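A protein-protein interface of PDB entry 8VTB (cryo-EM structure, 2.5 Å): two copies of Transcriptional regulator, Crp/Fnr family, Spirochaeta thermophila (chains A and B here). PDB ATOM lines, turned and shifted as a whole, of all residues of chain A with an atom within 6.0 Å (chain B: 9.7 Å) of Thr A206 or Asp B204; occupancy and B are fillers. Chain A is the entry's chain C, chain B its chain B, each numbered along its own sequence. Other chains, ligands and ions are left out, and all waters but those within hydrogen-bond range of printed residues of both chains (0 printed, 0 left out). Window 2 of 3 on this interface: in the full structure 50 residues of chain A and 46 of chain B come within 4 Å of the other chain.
The backbone carbonyl oxygen (O) of Tyr B191 lies within hydrogen-bond range of the side-chain hydroxyl (OG1) of Thr B195, 2.6 Å away.
OH of Tyr B191 sits at hydrogen-bond distance from OD2 of Asp B204, at 2.9 Å.
O of Gln A212 lies within hydrogen-bond range of OG1 of Thr A216 (2.6 Å).
Thr A206 touches Asp B204, but with the chains exchanged Asp A204 does not touch Thr B206 (11.5 Å).
Positions printed for both chains: 171, 192, 203, 204, 205, 206, 207 and 208.
Of the 6 pairs that touch across the chains among the printed residues, none has its exchanged pair printed and touching as well.
Thr A206 touches one residue of chain B.
Asp B204 touches just one residue of chain A: Thr A206.
Gly A203 touches just one residue of chain B: Tyr B202.
Pro A207 touches just one residue of chain B: Tyr B191.
Printed residues of chain A within 4 Å of Tyr B191: Pro A207 (3.3 Å) and Thr A216 (3.6 Å).
Printed residues of chain B within 4 Å of Trp A192: Tyr B202 (3.6 Å).
Of the printed residues of chain B, Thr A216 touches Tyr B191 and Tyr B202.
Of the printed residues of chain A, Tyr B202 touches Trp A192 (3.6 Å), Gly A203 (3.5 Å) and Thr A216 (3.9 Å).
Gln A212 touches none of the printed residues of chain B.
The nearest residue of chain A that does not touch Asp B204 is Pro A207 (4.8 Å).
The nearest printed residue of chain A that does not touch Tyr B191 is Thr A206 (4.1 Å).
Printed residues of chain A that touch a printed residue of chain B: Trp A192, Gly A203, Thr A206, Pro A207 and Thr A216.
Hydrophobic or aromatic side chains of chain A within 4 Å of the printed part of chain B: Trp A192 and Pro A207.
Along chain A the printed residues that touch a printed residue of chain B span positions 192 to 216.
Of the 19 printed residues of chain B, 3 touch a printed residue of chain A.
Printed residues of chain B that touch a printed residue of chain A: Tyr B191, Tyr B202 and Asp B204.
Trp A192 touches Tyr B202 (NE1 to OH, 3.6 Å).
Tyr B202 touches Gly A203 (CD1 to CA, 3.5 Å).
OD2 of Asp B204 touches CB of Thr A206, 3.7 Å away.
Pro A207 touches Tyr B191 (CD to OH, 3.3 Å).
Tyr B191 touches Thr A216.
Thr A216 touches Tyr B202.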
ATOM      1  N   TRP A 171      19.033   1.569 -21.097  1.00  0.00           N
ATOM      2  CA  TRP A 171      18.602   2.007 -22.419  1.00  0.00           C
ATOM      3  C   TRP A 171      19.487   1.413 -23.507  1.00  0.00           C
ATOM      4  O   TRP A 171      18.991   0.960 -24.548  1.00  0.00           O
ATOM      5  CB  TRP A 171      18.609   3.535 -22.479  1.00  0.00           C
ATOM      6  CG  TRP A 171      18.117   4.104 -23.768  1.00  0.00           C
ATOM      7  CD1 TRP A 171      18.875   4.645 -24.762  1.00  0.00           C
ATOM      8  CD2 TRP A 171      16.757   4.198 -24.206  1.00  0.00           C
ATOM      9  NE1 TRP A 171      18.076   5.068 -25.794  1.00  0.00           N
ATOM     10  CE2 TRP A 171      16.768   4.804 -25.476  1.00  0.00           C
ATOM     11  CE3 TRP A 171      15.531   3.828 -23.647  1.00  0.00           C
ATOM     12  CZ2 TRP A 171      15.605   5.047 -26.197  1.00  0.00           C
ATOM     13  CZ3 TRP A 171      14.377   4.070 -24.363  1.00  0.00           C
ATOM     14  CH2 TRP A 171      14.421   4.674 -25.626  1.00  0.00           C
ATOM     15  N   TRP A 192      19.558  10.801 -23.668  1.00  0.00           N
ATOM     16  CA  TRP A 192      18.146  10.454 -23.541  1.00  0.00           C
ATOM     17  C   TRP A 192      17.699  10.456 -22.084  1.00  0.00           C
ATOM     18  O   TRP A 192      16.641  11.003 -21.747  1.00  0.00           O
ATOM     19  CB  TRP A 192      17.875   9.089 -24.168  1.00  0.00           C
ATOM     20  CG  TRP A 192      16.489   8.613 -23.893  1.00  0.00           C
ATOM     21  CD1 TRP A 192      15.353   8.984 -24.546  1.00  0.00           C
ATOM     22  CD2 TRP A 192      16.078   7.709 -22.860  1.00  0.00           C
ATOM     23  NE1 TRP A 192      14.262   8.355 -23.999  1.00  0.00           N
ATOM     24  CE2 TRP A 192      14.683   7.566 -22.961  1.00  0.00           C
ATOM     25  CE3 TRP A 192      16.758   7.001 -21.867  1.00  0.00           C
ATOM     26  CZ2 TRP A 192      13.953   6.746 -22.108  1.00  0.00           C
ATOM     27  CZ3 TRP A 192      16.035   6.186 -21.021  1.00  0.00           C
ATOM     28  CH2 TRP A 192      14.645   6.064 -21.145  1.00  0.00           C
ATOM     29  N   GLY A 203      12.373  14.645 -27.344  1.00  0.00           N
ATOM     30  CA  GLY A 203      11.747  13.633 -28.167  1.00  0.00           C
ATOM     31  C   GLY A 203      12.475  13.309 -29.450  1.00  0.00           C
ATOM     32  O   GLY A 203      11.899  12.663 -30.328  1.00  0.00           O
ATOM     33  N   ASP A 204      13.730  13.739 -29.591  1.00  0.00           N
ATOM     34  CA  ASP A 204      14.517  13.326 -30.746  1.00  0.00           C
ATOM     35  C   ASP A 204      14.969  11.877 -30.621  1.00  0.00           C
ATOM     36  O   ASP A 204      15.201  11.213 -31.636  1.00  0.00           O
ATOM     37  CB  ASP A 204      15.721  14.249 -30.931  1.00  0.00           C
ATOM     38  CG  ASP A 204      16.598  14.316 -29.702  1.00  0.00           C
ATOM     39  OD1 ASP A 204      16.105  13.995 -28.600  1.00  0.00           O
ATOM     40  OD2 ASP A 204      17.782  14.689 -29.838  1.00  0.00           O
ATOM     41  N   ILE A 205      15.100  11.378 -29.395  1.00  0.00           N
ATOM     42  CA  ILE A 205      15.317   9.962 -29.122  1.00  0.00           C
ATOM     43  C   ILE A 205      14.092   9.441 -28.385  1.00  0.00           C
ATOM     44  O   ILE A 205      13.745   9.947 -27.311  1.00  0.00           O
ATOM     45  CB  ILE A 205      16.594   9.732 -28.296  1.00  0.00           C
ATOM     46  CG1 ILE A 205      17.809  10.318 -29.016  1.00  0.00           C
ATOM     47  CG2 ILE A 205      16.791   8.251 -28.025  1.00  0.00           C
ATOM     48  CD1 ILE A 205      19.069  10.299 -28.185  1.00  0.00           C
ATOM     49  N   THR A 206      13.444   8.431 -28.956  1.00  0.00           N
ATOM     50  CA  THR A 206      12.192   7.916 -28.421  1.00  0.00           C
ATOM     51  C   THR A 206      12.208   6.395 -28.540  1.00  0.00           C
ATOM     52  O   THR A 206      12.918   5.846 -29.380  1.00  0.00           O
ATOM     53  CB  THR A 206      10.978   8.493 -29.162  1.00  0.00           C
ATOM     54  OG1 THR A 206      11.127   8.294 -30.572  1.00  0.00           O
ATOM     55  CG2 THR A 206      10.813   9.979 -28.868  1.00  0.00           C
ATOM     56  N   PRO A 207      11.434   5.703 -27.701  1.00  0.00           N
ATOM     57  CA  PRO A 207      11.367   4.236 -27.809  1.00  0.00           C
ATOM     58  C   PRO A 207      10.713   3.807 -29.114  1.00  0.00           C
ATOM     59  O   PRO A 207       9.700   4.372 -29.533  1.00  0.00           O
ATOM     60  CB  PRO A 207      10.519   3.837 -26.594  1.00  0.00           C
ATOM     61  CG  PRO A 207       9.681   5.041 -26.327  1.00  0.00           C
ATOM     62  CD  PRO A 207      10.611   6.193 -26.589  1.00  0.00           C
ATOM     63  N   SER A 208      11.305   2.800 -29.757  1.00  0.00           N
ATOM     64  CA  SER A 208      10.792   2.272 -31.014  1.00  0.00           C
ATOM     65  C   SER A 208      10.148   0.898 -30.880  1.00  0.00           C
ATOM     66  O   SER A 208       9.517   0.435 -31.836  1.00  0.00           O
ATOM     67  CB  SER A 208      11.917   2.203 -32.053  1.00  0.00           C
ATOM     68  OG  SER A 208      12.470   3.485 -32.288  1.00  0.00           O
ATOM     69  N   GLN A 212      11.076  -1.157 -25.142  1.00  0.00           N
ATOM     70  CA  GLN A 212      11.594   0.189 -24.940  1.00  0.00           C
ATOM     71  C   GLN A 212      10.498   1.140 -24.489  1.00  0.00           C
ATOM     72  O   GLN A 212      10.765   2.061 -23.722  1.00  0.00           O
ATOM     73  CB  GLN A 212      12.256   0.713 -26.214  1.00  0.00           C
ATOM     74  CG  GLN A 212      13.519  -0.020 -26.619  1.00  0.00           C
ATOM     75  CD  GLN A 212      13.949   0.302 -28.037  1.00  0.00           C
ATOM     76  OE1 GLN A 212      13.480   1.270 -28.634  1.00  0.00           O
ATOM     77  NE2 GLN A 212      14.853  -0.504 -28.580  1.00  0.00           N
ATOM     78  N   THR A 216      10.579   3.142 -21.118  1.00  0.00           N
ATOM     79  CA  THR A 216      10.416   4.587 -21.172  1.00  0.00           C
ATOM     80  C   THR A 216       9.354   5.059 -20.192  1.00  0.00           C
ATOM     81  O   THR A 216       9.525   6.081 -19.530  1.00  0.00           O
ATOM     82  CB  THR A 216      10.067   5.018 -22.596  1.00  0.00           C
ATOM     83  OG1 THR A 216      11.125   4.637 -23.483  1.00  0.00           O
ATOM     84  CG2 THR A 216       9.875   6.526 -22.670  1.00  0.00           C
ATOM     85  N   TRP B 171      -7.947   8.047 -24.671  1.00  0.00           N
ATOM     86  CA  TRP B 171      -7.118   8.276 -25.849  1.00  0.00           C
ATOM     87  C   TRP B 171      -7.334   7.186 -26.891  1.00  0.00           C
ATOM     88  O   TRP B 171      -7.440   7.471 -28.092  1.00  0.00           O
ATOM     89  CB  TRP B 171      -5.649   8.355 -25.432  1.00  0.00           C
ATOM     90  CG  TRP B 171      -4.707   8.658 -26.551  1.00  0.00           C
ATOM     91  CD1 TRP B 171      -3.874   7.780 -27.177  1.00  0.00           C
ATOM     92  CD2 TRP B 171      -4.490   9.930 -27.173  1.00  0.00           C
ATOM     93  NE1 TRP B 171      -3.156   8.420 -28.154  1.00  0.00           N
ATOM     94  CE2 TRP B 171      -3.515   9.743 -28.171  1.00  0.00           C
ATOM     95  CE3 TRP B 171      -5.026  11.205 -26.985  1.00  0.00           C
ATOM     96  CZ2 TRP B 171      -3.066  10.783 -28.979  1.00  0.00           C
ATOM     97  CZ3 TRP B 171      -4.579  12.236 -27.786  1.00  0.00           C
ATOM     98  CH2 TRP B 171      -3.608  12.019 -28.772  1.00  0.00           C
ATOM     99  N   GLN B 175      -8.952   7.285 -30.811  1.00  0.00           N
ATOM    100  CA  GLN B 175      -8.031   6.927 -31.883  1.00  0.00           C
ATOM    101  C   GLN B 175      -8.786   6.329 -33.071  1.00  0.00           C
ATOM    102  O   GLN B 175      -9.815   5.673 -32.887  1.00  0.00           O
ATOM    103  CB  GLN B 175      -6.983   5.933 -31.386  1.00  0.00           C
ATOM    104  CG  GLN B 175      -5.746   6.563 -30.758  1.00  0.00           C
ATOM    105  CD  GLN B 175      -5.319   7.852 -31.435  1.00  0.00           C
ATOM    106  OE1 GLN B 175      -4.568   7.834 -32.410  1.00  0.00           O
ATOM    107  NE2 GLN B 175      -5.779   8.982 -30.905  1.00  0.00           N
ATOM    108  N   LEU B 187      -0.569   0.057 -24.810  1.00  0.00           N
ATOM    109  CA  LEU B 187       0.782   0.488 -24.471  1.00  0.00           C
ATOM    110  C   LEU B 187       1.081   1.866 -25.046  1.00  0.00           C
ATOM    111  O   LEU B 187       1.656   2.719 -24.360  1.00  0.00           O
ATOM    112  CB  LEU B 187       1.802  -0.532 -24.970  1.00  0.00           C
ATOM    113  CG  LEU B 187       3.260  -0.169 -24.690  1.00  0.00           C
ATOM    114  CD1 LEU B 187       3.510  -0.081 -23.197  1.00  0.00           C
ATOM    115  CD2 LEU B 187       4.190  -1.178 -25.326  1.00  0.00           C
ATOM    116  N   SER B 188       0.687   2.109 -26.298  1.00  0.00           N
ATOM    117  CA  SER B 188       0.917   3.418 -26.903  1.00  0.00           C
ATOM    118  C   SER B 188       0.113   4.505 -26.198  1.00  0.00           C
ATOM    119  O   SER B 188       0.626   5.603 -25.951  1.00  0.00           O
ATOM    120  CB  SER B 188       0.574   3.376 -28.391  1.00  0.00           C
ATOM    121  OG  SER B 188       1.305   2.363 -29.057  1.00  0.00           O
ATOM    122  N   TYR B 191       1.714   5.158 -22.847  1.00  0.00           N
ATOM    123  CA  TYR B 191       2.939   5.910 -23.085  1.00  0.00           C
ATOM    124  C   TYR B 191       2.629   7.385 -23.303  1.00  0.00           C
ATOM    125  O   TYR B 191       3.270   8.260 -22.708  1.00  0.00           O
ATOM    126  CB  TYR B 191       3.672   5.313 -24.285  1.00  0.00           C
ATOM    127  CG  TYR B 191       4.842   6.117 -24.801  1.00  0.00           C
ATOM    128  CD1 TYR B 191       5.787   6.655 -23.937  1.00  0.00           C
ATOM    129  CD2 TYR B 191       5.009   6.325 -26.162  1.00  0.00           C
ATOM    130  CE1 TYR B 191       6.857   7.387 -24.415  1.00  0.00           C
ATOM    131  CE2 TYR B 191       6.074   7.053 -26.651  1.00  0.00           C
ATOM    132  CZ  TYR B 191       6.993   7.581 -25.775  1.00  0.00           C
ATOM    133  OH  TYR B 191       8.058   8.308 -26.259  1.00  0.00           O
ATOM    134  N   TRP B 192       1.628   7.679 -24.135  1.00  0.00           N
ATOM    135  CA  TRP B 192       1.250   9.067 -24.376  1.00  0.00           C
ATOM    136  C   TRP B 192       0.790   9.752 -23.094  1.00  0.00           C
ATOM    137  O   TRP B 192       1.196  10.884 -22.800  1.00  0.00           O
ATOM    138  CB  TRP B 192       0.149   9.143 -25.432  1.00  0.00           C
ATOM    139  CG  TRP B 192      -0.400  10.523 -25.568  1.00  0.00           C
ATOM    140  CD1 TRP B 192       0.151  11.555 -26.268  1.00  0.00           C
ATOM    141  CD2 TRP B 192      -1.585  11.043 -24.956  1.00  0.00           C
ATOM    142  NE1 TRP B 192      -0.627  12.680 -26.146  1.00  0.00           N
ATOM    143  CE2 TRP B 192      -1.698  12.390 -25.344  1.00  0.00           C
ATOM    144  CE3 TRP B 192      -2.566  10.496 -24.124  1.00  0.00           C
ATOM    145  CZ2 TRP B 192      -2.751  13.199 -24.930  1.00  0.00           C
ATOM    146  CZ3 TRP B 192      -3.609  11.299 -23.714  1.00  0.00           C
ATOM    147  CH2 TRP B 192      -3.695  12.637 -24.116  1.00  0.00           C
ATOM    148  N   THR B 193      -0.074   9.086 -22.319  1.00  0.00           N
ATOM    149  CA  THR B 193      -0.638   9.747 -21.144  1.00  0.00           C
ATOM    150  C   THR B 193       0.416   9.946 -20.060  1.00  0.00           C
ATOM    151  O   THR B 193       0.389  10.955 -19.348  1.00  0.00           O
ATOM    152  CB  THR B 193      -1.851   8.981 -20.603  1.00  0.00           C
ATOM    153  OG1 THR B 193      -2.412   9.701 -19.499  1.00  0.00           O
ATOM    154  CG2 THR B 193      -1.470   7.606 -20.123  1.00  0.00           C
ATOM    155  N   ILE B 194       1.348   9.001 -19.910  1.00  0.00           N
ATOM    156  CA  ILE B 194       2.439   9.196 -18.961  1.00  0.00           C
ATOM    157  C   ILE B 194       3.360  10.311 -19.436  1.00  0.00           C
ATOM    158  O   ILE B 194       3.828  11.130 -18.637  1.00  0.00           O
ATOM    159  CB  ILE B 194       3.204   7.878 -18.741  1.00  0.00           C
ATOM    160  CG1 ILE B 194       2.301   6.844 -18.072  1.00  0.00           C
ATOM    161  CG2 ILE B 194       4.449   8.110 -17.897  1.00  0.00           C
ATOM    162  CD1 ILE B 194       1.657   7.331 -16.798  1.00  0.00           C
ATOM    163  N   THR B 195       3.627  10.369 -20.744  1.00  0.00           N
ATOM    164  CA  THR B 195       4.465  11.430 -21.287  1.00  0.00           C
ATOM    165  C   THR B 195       3.839  12.800 -21.052  1.00  0.00           C
ATOM    166  O   THR B 195       4.548  13.783 -20.808  1.00  0.00           O
ATOM    167  CB  THR B 195       4.697  11.186 -22.780  1.00  0.00           C
ATOM    168  OG1 THR B 195       5.276   9.890 -22.967  1.00  0.00           O
ATOM    169  CG2 THR B 195       5.639  12.224 -23.351  1.00  0.00           C
ATOM    170  N   THR B 196       2.511  12.883 -21.108  1.00  0.00           N
ATOM    171  CA  THR B 196       1.817  14.152 -20.905  1.00  0.00           C
ATOM    172  C   THR B 196       1.705  14.528 -19.429  1.00  0.00           C
ATOM    173  O   THR B 196       1.976  15.674 -19.059  1.00  0.00           O
ATOM    174  CB  THR B 196       0.420  14.099 -21.532  1.00  0.00           C
ATOM    175  OG1 THR B 196       0.527  13.736 -22.913  1.00  0.00           O
ATOM    176  CG2 THR B 196      -0.273  15.446 -21.408  1.00  0.00           C
ATOM    177  N   ILE B 200       6.822  15.669 -19.565  1.00  0.00           N
ATOM    178  CA  ILE B 200       8.033  15.471 -20.352  1.00  0.00           C
ATOM    179  C   ILE B 200       7.785  15.838 -21.810  1.00  0.00           C
ATOM    180  O   ILE B 200       8.559  16.590 -22.415  1.00  0.00           O
ATOM    181  CB  ILE B 200       8.545  14.028 -20.196  1.00  0.00           C
ATOM    182  CG1 ILE B 200       8.978  13.794 -18.748  1.00  0.00           C
ATOM    183  CG2 ILE B 200       9.693  13.761 -21.148  1.00  0.00           C
ATOM    184  CD1 ILE B 200       9.227  12.359 -18.399  1.00  0.00           C
ATOM    185  N   GLY B 201       6.697  15.334 -22.389  1.00  0.00           N
ATOM    186  CA  GLY B 201       6.253  15.794 -23.692  1.00  0.00           C
ATOM    187  C   GLY B 201       7.193  15.565 -24.859  1.00  0.00           C
ATOM    188  O   GLY B 201       7.598  16.531 -25.513  1.00  0.00           O
ATOM    189  N   TYR B 202       7.571  14.308 -25.123  1.00  0.00           N
ATOM    190  CA  TYR B 202       8.376  14.020 -26.308  1.00  0.00           C
ATOM    191  C   TYR B 202       7.704  14.498 -27.585  1.00  0.00           C
ATOM    192  O   TYR B 202       8.380  14.977 -28.502  1.00  0.00           O
ATOM    193  CB  TYR B 202       8.663  12.522 -26.428  1.00  0.00           C
ATOM    194  CG  TYR B 202       9.467  11.924 -25.301  1.00  0.00           C
ATOM    195  CD1 TYR B 202      10.729  12.407 -24.995  1.00  0.00           C
ATOM    196  CD2 TYR B 202       8.987  10.841 -24.580  1.00  0.00           C
ATOM    197  CE1 TYR B 202      11.478  11.854 -23.981  1.00  0.00           C
ATOM    198  CE2 TYR B 202       9.728  10.279 -23.564  1.00  0.00           C
ATOM    199  CZ  TYR B 202      10.972  10.789 -23.269  1.00  0.00           C
ATOM    200  OH  TYR B 202      11.715  10.233 -22.257  1.00  0.00           O
ATOM    201  N   GLY B 203       6.382  14.374 -27.671  1.00  0.00           N
ATOM    202  CA  GLY B 203       5.677  14.787 -28.864  1.00  0.00           C
ATOM    203  C   GLY B 203       5.777  13.836 -30.033  1.00  0.00           C
ATOM    204  O   GLY B 203       5.437  14.214 -31.156  1.00  0.00           O
ATOM    205  N   ASP B 204       6.238  12.605 -29.806  1.00  0.00           N
ATOM    206  CA  ASP B 204       6.215  11.611 -30.873  1.00  0.00           C
ATOM    207  C   ASP B 204       4.804  11.096 -31.121  1.00  0.00           C
ATOM    208  O   ASP B 204       4.494  10.656 -32.233  1.00  0.00           O
ATOM    209  CB  ASP B 204       7.158  10.453 -30.545  1.00  0.00           C
ATOM    210  CG  ASP B 204       6.841   9.801 -29.220  1.00  0.00           C
ATOM    211  OD1 ASP B 204       6.187  10.450 -28.378  1.00  0.00           O
ATOM    212  OD2 ASP B 204       7.246   8.636 -29.020  1.00  0.00           O
ATOM    213  N   ILE B 205       3.945  11.141 -30.106  1.00  0.00           N
ATOM    214  CA  ILE B 205       2.518  10.884 -30.248  1.00  0.00           C
ATOM    215  C   ILE B 205       1.782  12.180 -29.941  1.00  0.00           C
ATOM    216  O   ILE B 205       1.923  12.733 -28.843  1.00  0.00           O
ATOM    217  CB  ILE B 205       2.048   9.752 -29.320  1.00  0.00           C
ATOM    218  CG1 ILE B 205       2.840   8.473 -29.593  1.00  0.00           C
ATOM    219  CG2 ILE B 205       0.559   9.510 -29.487  1.00  0.00           C
ATOM    220  CD1 ILE B 205       2.569   7.371 -28.598  1.00  0.00           C
ATOM    221  N   THR B 206       0.999  12.659 -30.900  1.00  0.00           N
ATOM    222  CA  THR B 206       0.332  13.948 -30.783  1.00  0.00           C
ATOM    223  C   THR B 206      -1.075  13.817 -31.361  1.00  0.00           C
ATOM    224  O   THR B 206      -1.327  12.942 -32.187  1.00  0.00           O
ATOM    225  CB  THR B 206       1.105  15.054 -31.515  1.00  0.00           C
ATOM    226  OG1 THR B 206       1.360  14.658 -32.866  1.00  0.00           O
ATOM    227  CG2 THR B 206       2.422  15.359 -30.812  1.00  0.00           C
ATOM    228  N   PRO B 207      -2.000  14.675 -30.928  1.00  0.00           N
ATOM    229  CA  PRO B 207      -3.359  14.631 -31.493  1.00  0.00           C
ATOM    230  C   PRO B 207      -3.361  15.028 -32.961  1.00  0.00           C
ATOM    231  O   PRO B 207      -2.701  15.989 -33.360  1.00  0.00           O
ATOM    232  CB  PRO B 207      -4.126  15.644 -30.632  1.00  0.00           C
ATOM    233  CG  PRO B 207      -3.072  16.589 -30.162  1.00  0.00           C
ATOM    234  CD  PRO B 207      -1.890  15.702 -29.885  1.00  0.00           C
ATOM    235  N   SER B 208      -4.112  14.275 -33.767  1.00  0.00           N
ATOM    236  CA  SER B 208      -4.220  14.535 -35.194  1.00  0.00           C
ATOM    237  C   SER B 208      -5.571  15.106 -35.608  1.00  0.00           C
ATOM    238  O   SER B 208      -5.714  15.536 -36.758  1.00  0.00           O
ATOM    239  CB  SER B 208      -3.951  13.250 -35.986  1.00  0.00           C
ATOM    240  OG  SER B 208      -2.656  12.747 -35.712  1.00  0.00           O
